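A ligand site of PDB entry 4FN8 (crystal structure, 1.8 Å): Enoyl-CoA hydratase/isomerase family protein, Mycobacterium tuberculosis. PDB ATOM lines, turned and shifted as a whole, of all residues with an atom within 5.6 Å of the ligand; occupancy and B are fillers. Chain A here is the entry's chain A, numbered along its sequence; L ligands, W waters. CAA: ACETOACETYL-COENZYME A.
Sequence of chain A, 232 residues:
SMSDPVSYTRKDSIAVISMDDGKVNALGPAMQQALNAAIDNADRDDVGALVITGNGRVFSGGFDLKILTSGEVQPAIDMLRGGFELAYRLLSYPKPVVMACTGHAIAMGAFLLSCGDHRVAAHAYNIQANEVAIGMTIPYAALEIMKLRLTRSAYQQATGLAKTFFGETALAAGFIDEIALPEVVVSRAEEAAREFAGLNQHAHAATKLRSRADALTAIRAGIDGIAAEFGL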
ATOM      1  N   LYS A  23     -20.484  -8.591  13.274  1.00  0.00           N
ATOM      2  CA  LYS A  23     -19.970  -8.320  14.618  1.00  0.00           C
ATOM      3  C   LYS A  23     -18.807  -7.306  14.567  1.00  0.00           C
ATOM      4  O   LYS A  23     -19.036  -6.144  14.227  1.00  0.00           O
ATOM      5  CB  LYS A  23     -19.551  -9.621  15.316  1.00  0.00           C
ATOM      6  CG  LYS A  23     -19.540  -9.487  16.841  1.00  0.00           C
ATOM      7  CD  LYS A  23     -19.374 -10.821  17.544  1.00  0.00           C
ATOM      8  CE  LYS A  23     -19.511 -10.641  19.058  1.00  0.00           C
ATOM      9  NZ  LYS A  23     -19.325 -11.925  19.796  1.00  0.00           N
ATOM     10  N   VAL A  24     -17.600  -7.735  14.891  1.00  0.00           N
ATOM     11  CA  VAL A  24     -16.456  -6.814  14.889  1.00  0.00           C
ATOM     12  C   VAL A  24     -15.398  -7.088  13.800  1.00  0.00           C
ATOM     13  O   VAL A  24     -14.228  -6.725  13.941  1.00  0.00           O
ATOM     14  CB  VAL A  24     -15.771  -6.737  16.279  1.00  0.00           C
ATOM     15  CG1 VAL A  24     -16.735  -6.149  17.311  1.00  0.00           C
ATOM     16  CG2 VAL A  24     -15.278  -8.107  16.717  1.00  0.00           C
ATOM     17  N   ALA A  26     -13.704  -9.635  12.785  1.00  0.00           N
ATOM     18  CA  ALA A  26     -12.523 -10.404  13.184  1.00  0.00           C
ATOM     19  C   ALA A  26     -11.827 -10.969  11.951  1.00  0.00           C
ATOM     20  O   ALA A  26     -12.490 -11.512  11.055  1.00  0.00           O
ATOM     21  CB  ALA A  26     -12.939 -11.530  14.138  1.00  0.00           C
ATOM     22  N   ARG A  57     -20.049  -0.619  13.098  1.00  0.00           N
ATOM     23  CA  ARG A  57     -19.590  -0.787  14.475  1.00  0.00           C
ATOM     24  C   ARG A  57     -18.073  -0.601  14.610  1.00  0.00           C
ATOM     25  O   ARG A  57     -17.591   0.016  15.570  1.00  0.00           O
ATOM     26  CB  ARG A  57     -19.986  -2.182  14.966  1.00  0.00           C
ATOM     27  CG  ARG A  57     -19.624  -2.487  16.421  1.00  0.00           C
ATOM     28  CD  ARG A  57     -20.171  -3.863  16.807  1.00  0.00           C
ATOM     29  NE  ARG A  57     -19.905  -4.198  18.201  1.00  0.00           N
ATOM     30  CZ  ARG A  57     -20.417  -5.263  18.827  1.00  0.00           C
ATOM     31  NH1 ARG A  57     -21.230  -6.085  18.189  1.00  0.00           N
ATOM     32  NH2 ARG A  57     -20.121  -5.484  20.103  1.00  0.00           N
ATOM     33  N   VAL A  58     -17.318  -1.165  13.664  1.00  0.00           N
ATOM     34  CA  VAL A  58     -15.850  -1.072  13.679  1.00  0.00           C
ATOM     35  C   VAL A  58     -15.284  -1.024  12.264  1.00  0.00           C
ATOM     36  O   VAL A  58     -15.989  -1.306  11.287  1.00  0.00           O
ATOM     37  CB  VAL A  58     -15.202  -2.311  14.347  1.00  0.00           C
ATOM     38  CG1 VAL A  58     -15.594  -2.412  15.826  1.00  0.00           C
ATOM     39  CG2 VAL A  58     -15.576  -3.584  13.586  1.00  0.00           C
ATOM     40  N   SER A  60     -12.177  -2.842  12.151  1.00  0.00           N
ATOM     41  CA  SER A  60     -11.973  -4.239  12.554  1.00  0.00           C
ATOM     42  C   SER A  60     -11.369  -4.298  13.942  1.00  0.00           C
ATOM     43  O   SER A  60     -10.497  -3.503  14.283  1.00  0.00           O
ATOM     44  CB  SER A  60     -11.085  -5.005  11.572  1.00  0.00           C
ATOM     45  OG  SER A  60     -10.648  -6.235  12.156  1.00  0.00           O
ATOM     46  N   GLY A  61     -11.850  -5.249  14.748  1.00  0.00           N
ATOM     47  CA  GLY A  61     -11.306  -5.515  16.063  1.00  0.00           C
ATOM     48  C   GLY A  61     -10.048  -6.374  16.064  1.00  0.00           C
ATOM     49  O   GLY A  61      -9.559  -6.740  17.134  1.00  0.00           O
ATOM     50  N   GLY A  62      -9.526  -6.695  14.880  1.00  0.00           N
ATOM     51  CA  GLY A  62      -8.259  -7.419  14.771  1.00  0.00           C
ATOM     52  C   GLY A  62      -8.426  -8.914  14.490  1.00  0.00           C
ATOM     53  O   GLY A  62      -9.477  -9.338  14.030  1.00  0.00           O
ATOM     54  N   PHE A  63      -7.383  -9.693  14.779  1.00  0.00           N
ATOM     55  CA  PHE A  63      -7.431 -11.143  14.583  1.00  0.00           C
ATOM     56  C   PHE A  63      -8.501 -11.753  15.481  1.00  0.00           C
ATOM     57  O   PHE A  63      -8.845 -11.187  16.503  1.00  0.00           O
ATOM     58  CB  PHE A  63      -6.079 -11.781  14.921  1.00  0.00           C
ATOM     59  CG  PHE A  63      -5.015 -11.582  13.858  1.00  0.00           C
ATOM     60  CD1 PHE A  63      -3.805 -10.978  14.164  1.00  0.00           C
ATOM     61  CD2 PHE A  63      -5.235 -11.996  12.548  1.00  0.00           C
ATOM     62  CE1 PHE A  63      -2.822 -10.809  13.206  1.00  0.00           C
ATOM     63  CE2 PHE A  63      -4.256 -11.827  11.580  1.00  0.00           C
ATOM     64  CZ  PHE A  63      -3.053 -11.237  11.910  1.00  0.00           C
ATOM     65  N   ASP A  64      -9.003 -12.929  15.084  1.00  0.00           N
ATOM     66  CA  ASP A  64      -9.981 -13.671  15.875  1.00  0.00           C
ATOM     67  C   ASP A  64      -9.359 -14.133  17.185  1.00  0.00           C
ATOM     68  O   ASP A  64      -8.495 -15.007  17.199  1.00  0.00           O
ATOM     69  CB  ASP A  64     -10.464 -14.890  15.068  1.00  0.00           C
ATOM     70  CG  ASP A  64     -11.603 -15.620  15.746  1.00  0.00           C
ATOM     71  OD1 ASP A  64     -11.839 -15.372  16.945  1.00  0.00           O
ATOM     72  OD2 ASP A  64     -12.252 -16.446  15.081  1.00  0.00           O
ATOM     73  N   LEU A  65      -9.800 -13.549  18.295  1.00  0.00           N
ATOM     74  CA  LEU A  65      -9.260 -13.893  19.612  1.00  0.00           C
ATOM     75  C   LEU A  65      -9.533 -15.348  20.006  1.00  0.00           C
ATOM     76  O   LEU A  65      -8.764 -15.949  20.754  1.00  0.00           O
ATOM     77  CB  LEU A  65      -9.812 -12.943  20.685  1.00  0.00           C
ATOM     78  CG  LEU A  65      -9.271 -11.510  20.663  1.00  0.00           C
ATOM     79  CD1 LEU A  65     -10.051 -10.621  21.638  1.00  0.00           C
ATOM     80  CD2 LEU A  65      -7.786 -11.495  20.991  1.00  0.00           C
ATOM     81  N   LYS A  66     -10.644 -15.894  19.516  1.00  0.00           N
ATOM     82  CA  LYS A  66     -10.978 -17.287  19.804  1.00  0.00           C
ATOM     83  C   LYS A  66      -9.878 -18.205  19.277  1.00  0.00           C
ATOM     84  O   LYS A  66      -9.371 -19.079  19.993  1.00  0.00           O
ATOM     85  CB  LYS A  66     -12.330 -17.653  19.196  1.00  0.00           C
ATOM     86  N   LEU A  68      -6.851 -17.245  18.367  1.00  0.00           N
ATOM     87  CA  LEU A  68      -5.590 -16.845  18.953  1.00  0.00           C
ATOM     88  C   LEU A  68      -5.360 -17.542  20.288  1.00  0.00           C
ATOM     89  O   LEU A  68      -4.239 -17.965  20.601  1.00  0.00           O
ATOM     90  CB  LEU A  68      -5.536 -15.324  19.126  1.00  0.00           C
ATOM     91  CG  LEU A  68      -4.266 -14.604  18.687  1.00  0.00           C
ATOM     92  CD1 LEU A  68      -4.235 -13.190  19.273  1.00  0.00           C
ATOM     93  CD2 LEU A  68      -3.011 -15.379  19.061  1.00  0.00           C
ATOM     94  N   LEU A  80      -2.126 -15.546  11.776  1.00  0.00           N
ATOM     95  CA  LEU A  80      -1.250 -14.376  11.794  1.00  0.00           C
ATOM     96  C   LEU A  80      -0.499 -14.197  10.483  1.00  0.00           C
ATOM     97  O   LEU A  80      -0.407 -13.091   9.964  1.00  0.00           O
ATOM     98  CB  LEU A  80      -0.270 -14.428  12.973  1.00  0.00           C
ATOM     99  CG  LEU A  80      -0.716 -13.674  14.243  1.00  0.00           C
ATOM    100  CD1 LEU A  80      -2.050 -14.203  14.746  1.00  0.00           C
ATOM    101  CD2 LEU A  80       0.347 -13.759  15.340  1.00  0.00           C
ATOM    102  N   PHE A  84      -0.754 -10.869   7.886  1.00  0.00           N
ATOM    103  CA  PHE A  84       0.384 -10.039   7.462  1.00  0.00           C
ATOM    104  C   PHE A  84       0.665 -10.202   5.971  1.00  0.00           C
ATOM    105  O   PHE A  84       1.177  -9.279   5.336  1.00  0.00           O
ATOM    106  CB  PHE A  84       1.607 -10.277   8.364  1.00  0.00           C
ATOM    107  CG  PHE A  84       1.383  -9.816   9.780  1.00  0.00           C
ATOM    108  CD1 PHE A  84       1.144  -8.470  10.048  1.00  0.00           C
ATOM    109  CD2 PHE A  84       1.396 -10.700  10.833  1.00  0.00           C
ATOM    110  CE1 PHE A  84       0.911  -8.037  11.350  1.00  0.00           C
ATOM    111  CE2 PHE A  84       1.170 -10.275  12.133  1.00  0.00           C
ATOM    112  CZ  PHE A  84       0.934  -8.936  12.389  1.00  0.00           C
ATOM    113  N   HIS A 104     -13.854   1.754  15.133  1.00  0.00           N
ATOM    114  CA  HIS A 104     -12.585   1.496  15.806  1.00  0.00           C
ATOM    115  C   HIS A 104     -11.722   0.524  15.015  1.00  0.00           C
ATOM    116  O   HIS A 104     -12.254  -0.349  14.319  1.00  0.00           O
ATOM    117  CB  HIS A 104     -12.828   0.932  17.214  1.00  0.00           C
ATOM    118  CG  HIS A 104     -13.820   1.703  18.011  1.00  0.00           C
ATOM    119  ND1 HIS A 104     -13.673   3.050  18.289  1.00  0.00           N
ATOM    120  CD2 HIS A 104     -14.990   1.325  18.581  1.00  0.00           C
ATOM    121  CE1 HIS A 104     -14.692   3.460  19.013  1.00  0.00           C
ATOM    122  NE2 HIS A 104     -15.513   2.432  19.197  1.00  0.00           N
ATOM    123  N   ILE A 106      -8.535  -1.895  15.949  1.00  0.00           N
ATOM    124  CA  ILE A 106      -7.691  -2.380  17.041  1.00  0.00           C
ATOM    125  C   ILE A 106      -6.734  -3.471  16.567  1.00  0.00           C
ATOM    126  O   ILE A 106      -7.141  -4.405  15.859  1.00  0.00           O
ATOM    127  CB  ILE A 106      -8.564  -2.965  18.176  1.00  0.00           C
ATOM    128  CG1 ILE A 106      -9.669  -1.976  18.566  1.00  0.00           C
ATOM    129  CG2 ILE A 106      -7.704  -3.351  19.400  1.00  0.00           C
ATOM    130  CD1 ILE A 106      -9.147  -0.650  19.135  1.00  0.00           C
ATOM    131  N   ALA A 107      -5.461  -3.332  16.939  1.00  0.00           N
ATOM    132  CA  ALA A 107      -4.439  -4.337  16.653  1.00  0.00           C
ATOM    133  C   ALA A 107      -4.365  -4.674  15.163  1.00  0.00           C
ATOM    134  O   ALA A 107      -4.063  -3.797  14.359  1.00  0.00           O
ATOM    135  CB  ALA A 107      -4.663  -5.580  17.528  1.00  0.00           C
ATOM    136  N   MET A 108      -4.598  -5.916  14.756  1.00  0.00           N
ATOM    137  CA  MET A 108      -4.529  -6.175  13.320  1.00  0.00           C
ATOM    138  C   MET A 108      -5.465  -5.267  12.502  1.00  0.00           C
ATOM    139  O   MET A 108      -5.212  -4.992  11.336  1.00  0.00           O
ATOM    140  CB  MET A 108      -4.764  -7.658  12.978  1.00  0.00           C
ATOM    141  CG  MET A 108      -4.457  -7.990  11.510  1.00  0.00           C
ATOM    142  SD  MET A 108      -2.692  -7.827  11.079  1.00  0.00           S
ATOM    143  CE  MET A 108      -2.821  -7.241   9.389  1.00  0.00           C
ATOM    144  N   GLY A 109      -6.545  -4.794  13.120  1.00  0.00           N
ATOM    145  CA  GLY A 109      -7.424  -3.850  12.440  1.00  0.00           C
ATOM    146  C   GLY A 109      -6.695  -2.541  12.139  1.00  0.00           C
ATOM    147  O   GLY A 109      -6.838  -1.949  11.060  1.00  0.00           O
ATOM    148  N   PHE A 111      -3.383  -2.339  11.938  1.00  0.00           N
ATOM    149  CA  PHE A 111      -2.281  -2.627  11.014  1.00  0.00           C
ATOM    150  C   PHE A 111      -2.816  -2.687   9.581  1.00  0.00           C
ATOM    151  O   PHE A 111      -2.180  -2.178   8.659  1.00  0.00           O
ATOM    152  CB  PHE A 111      -1.543  -3.914  11.406  1.00  0.00           C
ATOM    153  CG  PHE A 111      -1.178  -3.971  12.859  1.00  0.00           C
ATOM    154  CD1 PHE A 111      -0.825  -2.826  13.553  1.00  0.00           C
ATOM    155  CD2 PHE A 111      -1.214  -5.182  13.549  1.00  0.00           C
ATOM    156  CE1 PHE A 111      -0.518  -2.877  14.910  1.00  0.00           C
ATOM    157  CE2 PHE A 111      -0.911  -5.233  14.896  1.00  0.00           C
ATOM    158  CZ  PHE A 111      -0.564  -4.088  15.571  1.00  0.00           C
ATOM    159  N   ASN A 130      -3.247  -2.682  20.805  1.00  0.00           N
ATOM    160  CA  ASN A 130      -3.527  -2.908  22.213  1.00  0.00           C
ATOM    161  C   ASN A 130      -2.780  -4.096  22.803  1.00  0.00           C
ATOM    162  O   ASN A 130      -3.027  -4.484  23.935  1.00  0.00           O
ATOM    163  CB  ASN A 130      -5.022  -3.123  22.431  1.00  0.00           C
ATOM    164  CG  ASN A 130      -5.490  -4.468  21.907  1.00  0.00           C
ATOM    165  OD1 ASN A 130      -4.944  -4.980  20.928  1.00  0.00           O
ATOM    166  ND2 ASN A 130      -6.496  -5.041  22.547  1.00  0.00           N
ATOM    167  N   GLU A 131      -1.868  -4.664  22.023  1.00  0.00           N
ATOM    168  CA  GLU A 131      -1.201  -5.917  22.408  1.00  0.00           C
ATOM    169  C   GLU A 131      -0.639  -5.871  23.832  1.00  0.00           C
ATOM    170  O   GLU A 131      -0.904  -6.782  24.634  1.00  0.00           O
ATOM    171  CB  GLU A 131      -0.088  -6.268  21.406  1.00  0.00           C
ATOM    172  CG  GLU A 131      -0.571  -6.914  20.107  1.00  0.00           C
ATOM    173  CD  GLU A 131      -0.969  -5.924  19.032  1.00  0.00           C
ATOM    174  OE1 GLU A 131      -1.212  -4.734  19.324  1.00  0.00           O
ATOM    175  OE2 GLU A 131      -1.036  -6.334  17.858  1.00  0.00           O
ATOM    176  N   ILE A 134      -2.938  -6.188  26.665  1.00  0.00           N
ATOM    177  CA  ILE A 134      -3.537  -7.516  26.889  1.00  0.00           C
ATOM    178  C   ILE A 134      -2.516  -8.641  27.030  1.00  0.00           C
ATOM    179  O   ILE A 134      -2.859  -9.822  26.969  1.00  0.00           O
ATOM    180  CB  ILE A 134      -4.621  -7.855  25.835  1.00  0.00           C
ATOM    181  CG1 ILE A 134      -4.036  -7.906  24.425  1.00  0.00           C
ATOM    182  CG2 ILE A 134      -5.752  -6.832  25.883  1.00  0.00           C
ATOM    183  CD1 ILE A 134      -5.028  -8.385  23.371  1.00  0.00           C
ATOM    184  N   MET A 136       0.369  -9.289  25.192  1.00  0.00           N
ATOM    185  CA  MET A 136       1.075  -9.825  24.029  1.00  0.00           C
ATOM    186  C   MET A 136       2.158  -8.870  23.540  1.00  0.00           C
ATOM    187  O   MET A 136       2.017  -7.656  23.635  1.00  0.00           O
ATOM    188  CB  MET A 136       0.110 -10.134  22.890  1.00  0.00           C
ATOM    189  CG  MET A 136      -0.866 -11.236  23.268  1.00  0.00           C
ATOM    190  SD  MET A 136      -2.058 -11.627  21.977  1.00  0.00           S
ATOM    191  CE  MET A 136      -2.765 -10.015  21.689  1.00  0.00           C
ATOM    192  N   THR A 137       3.244  -9.448  23.037  1.00  0.00           N
ATOM    193  CA  THR A 137       4.306  -8.684  22.376  1.00  0.00           C
ATOM    194  C   THR A 137       3.875  -8.437  20.935  1.00  0.00           C
ATOM    195  O   THR A 137       3.266  -9.305  20.298  1.00  0.00           O
ATOM    196  CB  THR A 137       5.642  -9.456  22.390  1.00  0.00           C
ATOM    197  OG1 THR A 137       5.981  -9.804  23.737  1.00  0.00           O
ATOM    198  CG2 THR A 137       6.749  -8.599  21.797  1.00  0.00           C
ATOM    199  N   ILE A 138       4.188  -7.256  20.411  1.00  0.00           N
ATOM    200  CA  ILE A 138       3.816  -6.930  19.034  1.00  0.00           C
ATOM    201  C   ILE A 138       4.733  -7.647  18.030  1.00  0.00           C
ATOM    202  O   ILE A 138       5.937  -7.516  18.108  1.00  0.00           O
ATOM    203  CB  ILE A 138       3.884  -5.408  18.787  1.00  0.00           C
ATOM    204  CG1 ILE A 138       2.920  -4.679  19.744  1.00  0.00           C
ATOM    205  CG2 ILE A 138       3.521  -5.082  17.354  1.00  0.00           C
ATOM    206  CD1 ILE A 138       2.955  -3.143  19.615  1.00  0.00           C
ATOM    207  N   PRO A 139       4.141  -8.408  17.090  1.00  0.00           N
ATOM    208  CA  PRO A 139       4.937  -9.112  16.086  1.00  0.00           C
ATOM    209  C   PRO A 139       5.771  -8.140  15.261  1.00  0.00           C
ATOM    210  O   PRO A 139       5.337  -7.017  14.995  1.00  0.00           O
ATOM    211  CB  PRO A 139       3.879  -9.748  15.174  1.00  0.00           C
ATOM    212  CG  PRO A 139       2.672  -9.872  16.032  1.00  0.00           C
ATOM    213  CD  PRO A 139       2.695  -8.677  16.940  1.00  0.00           C
HETATM  214  N1A CAA L   1     -11.859 -11.546  17.968  1.00  0.00           N
HETATM  215  C2A CAA L   1     -13.082 -12.314  18.390  1.00  0.00           C
HETATM  216  N3A CAA L   1     -14.146 -11.601  19.192  1.00  0.00           N
HETATM  217  C4A CAA L   1     -13.957 -10.161  19.529  1.00  0.00           C
HETATM  218  C5A CAA L   1     -12.761  -9.408  19.116  1.00  0.00           C
HETATM  219  C6A CAA L   1     -11.679 -10.136  18.319  1.00  0.00           C
HETATM  220  N6A CAA L   1     -10.505  -9.411  17.883  1.00  0.00           N
HETATM  221  N7A CAA L   1     -12.860  -8.017  19.610  1.00  0.00           N
HETATM  222  C8A CAA L   1     -14.173  -7.889  20.356  1.00  0.00           C
HETATM  223  N9A CAA L   1     -14.810  -9.203  20.306  1.00  0.00           N
HETATM  224  C1B CAA L   1     -16.113  -9.598  20.840  1.00  0.00           C
HETATM  225  C2B CAA L   1     -16.152  -9.352  22.360  1.00  0.00           C
HETATM  226  O2B CAA L   1     -15.808 -10.562  22.999  1.00  0.00           O
HETATM  227  C3B CAA L   1     -17.621  -9.042  22.513  1.00  0.00           C
HETATM  228  O3B CAA L   1     -18.308 -10.258  22.289  1.00  0.00           O
HETATM  229  P3B CAA L   1     -19.704 -10.577  23.132  1.00  0.00           P
HETATM  230  O7A CAA L   1     -19.301 -11.270  24.574  1.00  0.00           O
HETATM  231  O8A CAA L   1     -20.508  -9.172  23.421  1.00  0.00           O
HETATM  232  O9A CAA L   1     -20.516 -11.498  22.324  1.00  0.00           O
HETATM  233  C4B CAA L   1     -17.875  -8.134  21.291  1.00  0.00           C
HETATM  234  O4B CAA L   1     -17.137  -8.762  20.192  1.00  0.00           O
HETATM  235  C5B CAA L   1     -17.228  -6.756  21.518  1.00  0.00           C
HETATM  236  O5B CAA L   1     -17.602  -6.312  22.807  1.00  0.00           O
HETATM  237  P1A CAA L   1     -17.697  -4.673  23.011  1.00  0.00           P
HETATM  238  O1A CAA L   1     -18.770  -4.307  24.211  1.00  0.00           O
HETATM  239  O2A CAA L   1     -16.359  -4.166  23.378  1.00  0.00           O
HETATM  240  O3A CAA L   1     -18.203  -4.046  21.552  1.00  0.00           O
HETATM  241  P2A CAA L   1     -17.679  -2.557  21.025  1.00  0.00           P
HETATM  242  O4A CAA L   1     -18.451  -2.246  19.601  1.00  0.00           O
HETATM  243  O5A CAA L   1     -17.988  -1.531  22.022  1.00  0.00           O
HETATM  244  O6A CAA L   1     -16.035  -2.608  20.787  1.00  0.00           O
HETATM  245  CBP CAA L   1     -13.969  -3.379  19.903  1.00  0.00           C
HETATM  246  CCP CAA L   1     -15.513  -3.403  19.724  1.00  0.00           C
HETATM  247  CDP CAA L   1     -13.473  -1.926  19.652  1.00  0.00           C
HETATM  248  CEP CAA L   1     -13.320  -4.356  18.891  1.00  0.00           C
HETATM  249  CAP CAA L   1     -13.635  -3.777  21.380  1.00  0.00           C
HETATM  250  OAP CAA L   1     -14.309  -4.965  21.735  1.00  0.00           O
HETATM  251  C9P CAA L   1     -12.131  -4.107  21.512  1.00  0.00           C
HETATM  252  O9P CAA L   1     -11.277  -3.298  21.339  1.00  0.00           O
HETATM  253  N8P CAA L   1     -11.818  -5.473  21.929  1.00  0.00           N
HETATM  254  C7P CAA L   1     -10.422  -5.891  22.090  1.00  0.00           C
HETATM  255  C6P CAA L   1      -9.996  -6.440  20.709  1.00  0.00           C
HETATM  256  C5P CAA L   1      -8.616  -7.098  20.771  1.00  0.00           C
HETATM  257  O5P CAA L   1      -8.148  -7.436  21.827  1.00  0.00           O
HETATM  258  N4P CAA L   1      -7.949  -7.374  19.493  1.00  0.00           N
HETATM  259  C3P CAA L   1      -6.655  -8.040  19.458  1.00  0.00           C
HETATM  260  C2P CAA L   1      -6.771  -9.159  18.402  1.00  0.00           C
HETATM  261  S1P CAA L   1      -5.122  -9.946  18.305  1.00  0.00           S
HETATM  262  C1  CAA L   1      -4.305  -9.243  16.829  1.00  0.00           C
HETATM  263  O1  CAA L   1      -5.190  -8.355  16.216  1.00  0.00           O
HETATM  264  C2  CAA L   1      -3.012  -8.496  17.168  1.00  0.00           C
HETATM  265  C3  CAA L   1      -1.842  -9.413  17.551  1.00  0.00           C
HETATM  266  O3  CAA L   1      -0.734  -8.966  17.565  1.00  0.00           O
HETATM  267  C4  CAA L   1      -2.105 -10.777  18.207  1.00  0.00           C
HETATM  268  O   HOH W   1     -15.586   0.462  22.402  1.00  0.00           O
HETATM  269  O   HOH W   2     -18.386   0.791  17.964  1.00  0.00           O
HETATM  270  O   HOH W   3     -15.299  -1.860  24.141  1.00  0.00           O
HETATM  271  O   HOH W   4      -9.152  -8.201  24.242  1.00  0.00           O
HETATM  272  O   HOH W   5     -21.084  -1.380  20.061  1.00  0.00           O
HETATM  273  O   HOH W   6      -3.516  -7.433  20.518  1.00  0.00           O
HETATM  274  O   HOH W   7     -16.631 -12.747  19.091  1.00  0.00           O
HETATM  275  O   HOH W   8     -13.281  -7.619  23.445  1.00  0.00           O
HETATM  276  O   HOH W   9     -21.841  -7.903  21.182  1.00  0.00           O
HETATM  277  O   HOH W  10     -11.129  -0.848  22.396  1.00  0.00           O
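O1 of the ligand lies within hydrogen-bond range of N of Met 108, 2.9 Å away.
O of Phe 63 lies within hydrogen-bond range of N6A of the ligand (2.8 Å).
NZ of Lys 23 lies within salt-bridge range of O9A of the ligand (2.8 Å).
N of Leu 65 lies within hydrogen-bond range of N1A of the ligand (2.9 Å).
The side-chain carboxylate (OE2) of Glu 131 lies close to an oxygen (O3) of the ligand (2.7 Å).
The side-chain amide nitrogen of Asn 130 lies within hydrogen-bond range of an oxygen (O5P) of the ligand, at 3.0 Å.
The backbone carbonyl oxygen (O) of Gly 61 lies within hydrogen-bond range of a nitrogen (N4P) of the ligand, 2.9 Å away.
The guanidinium group of Arg 57 is in salt-bridge range of an oxygen (O4A) of the ligand, at 2.8 Å.
O1 of the ligand lies within hydrogen-bond range of N of Phe 63, at 2.9 Å.
Residues that only touch the ligand: Ala 107, Leu 68, Ile 106, Pro 139, Gly 62, Asp 64, Ile 134, Met 136, Val 24, His 104 and Ala 26.
Hydrophobic or aromatic side chains within 4 Å of the ligand: Val 24, Ala 26, Phe 63, Leu 65, Leu 68, His 104, Ile 106, Ala 107, Met 108, Ile 134, Met 136 and Pro 139.
Within 4 Å of the ligand: Lys 23, Val 24, Ala 26, Arg 57, Gly 61, Gly 62, Phe 63, Asp 64, Leu 65, Leu 68, His 104, Ile 106, Ala 107, Met 108, Asn 130, Glu 131, Ile 134, Met 136 and Pro 139.
The backbone NH (N) of Gly 61 sits at hydrogen-bond distance from the backbone carbonyl oxygen (O) of Val 24, 2.9 Å away.
The backbone NH (N) of Ile 106 is in hydrogen-bond range of the backbone carbonyl oxygen (O) of Ser 60.
O of Ile 106 lies close to N of Gly 62 (3.4 Å).
The backbone carbonyl oxygen of His 104 lies within hydrogen-bond range of the backbone NH of Ser 60, at 3.3 Å.
OD1 of Asp 64 lies within hydrogen-bond range of N of Lys 66 (2.9 Å).
O of Glu 131 lies within hydrogen-bond range of N of Met 136 (2.9 Å).
N of Gly 62 lies within hydrogen-bond range of OG of Ser 60 (3.0 Å).
Water W7 bridges a nitrogen (N3A) of the ligand (2.7 Å) and the side-chain amino group of Lys 23 (2.9 Å).
Water W9 lies within hydrogen-bond range of O8A of the ligand (2.9 Å) and NH2 of Arg 57 (3.2 Å).
Water W6 bridges OD1 of Asn 130 (2.9 Å) and S1P of the ligand (3.7 Å).
Water W2 bridges O of Arg 57 (2.6 Å) and O4A of the ligand (3.5 Å).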
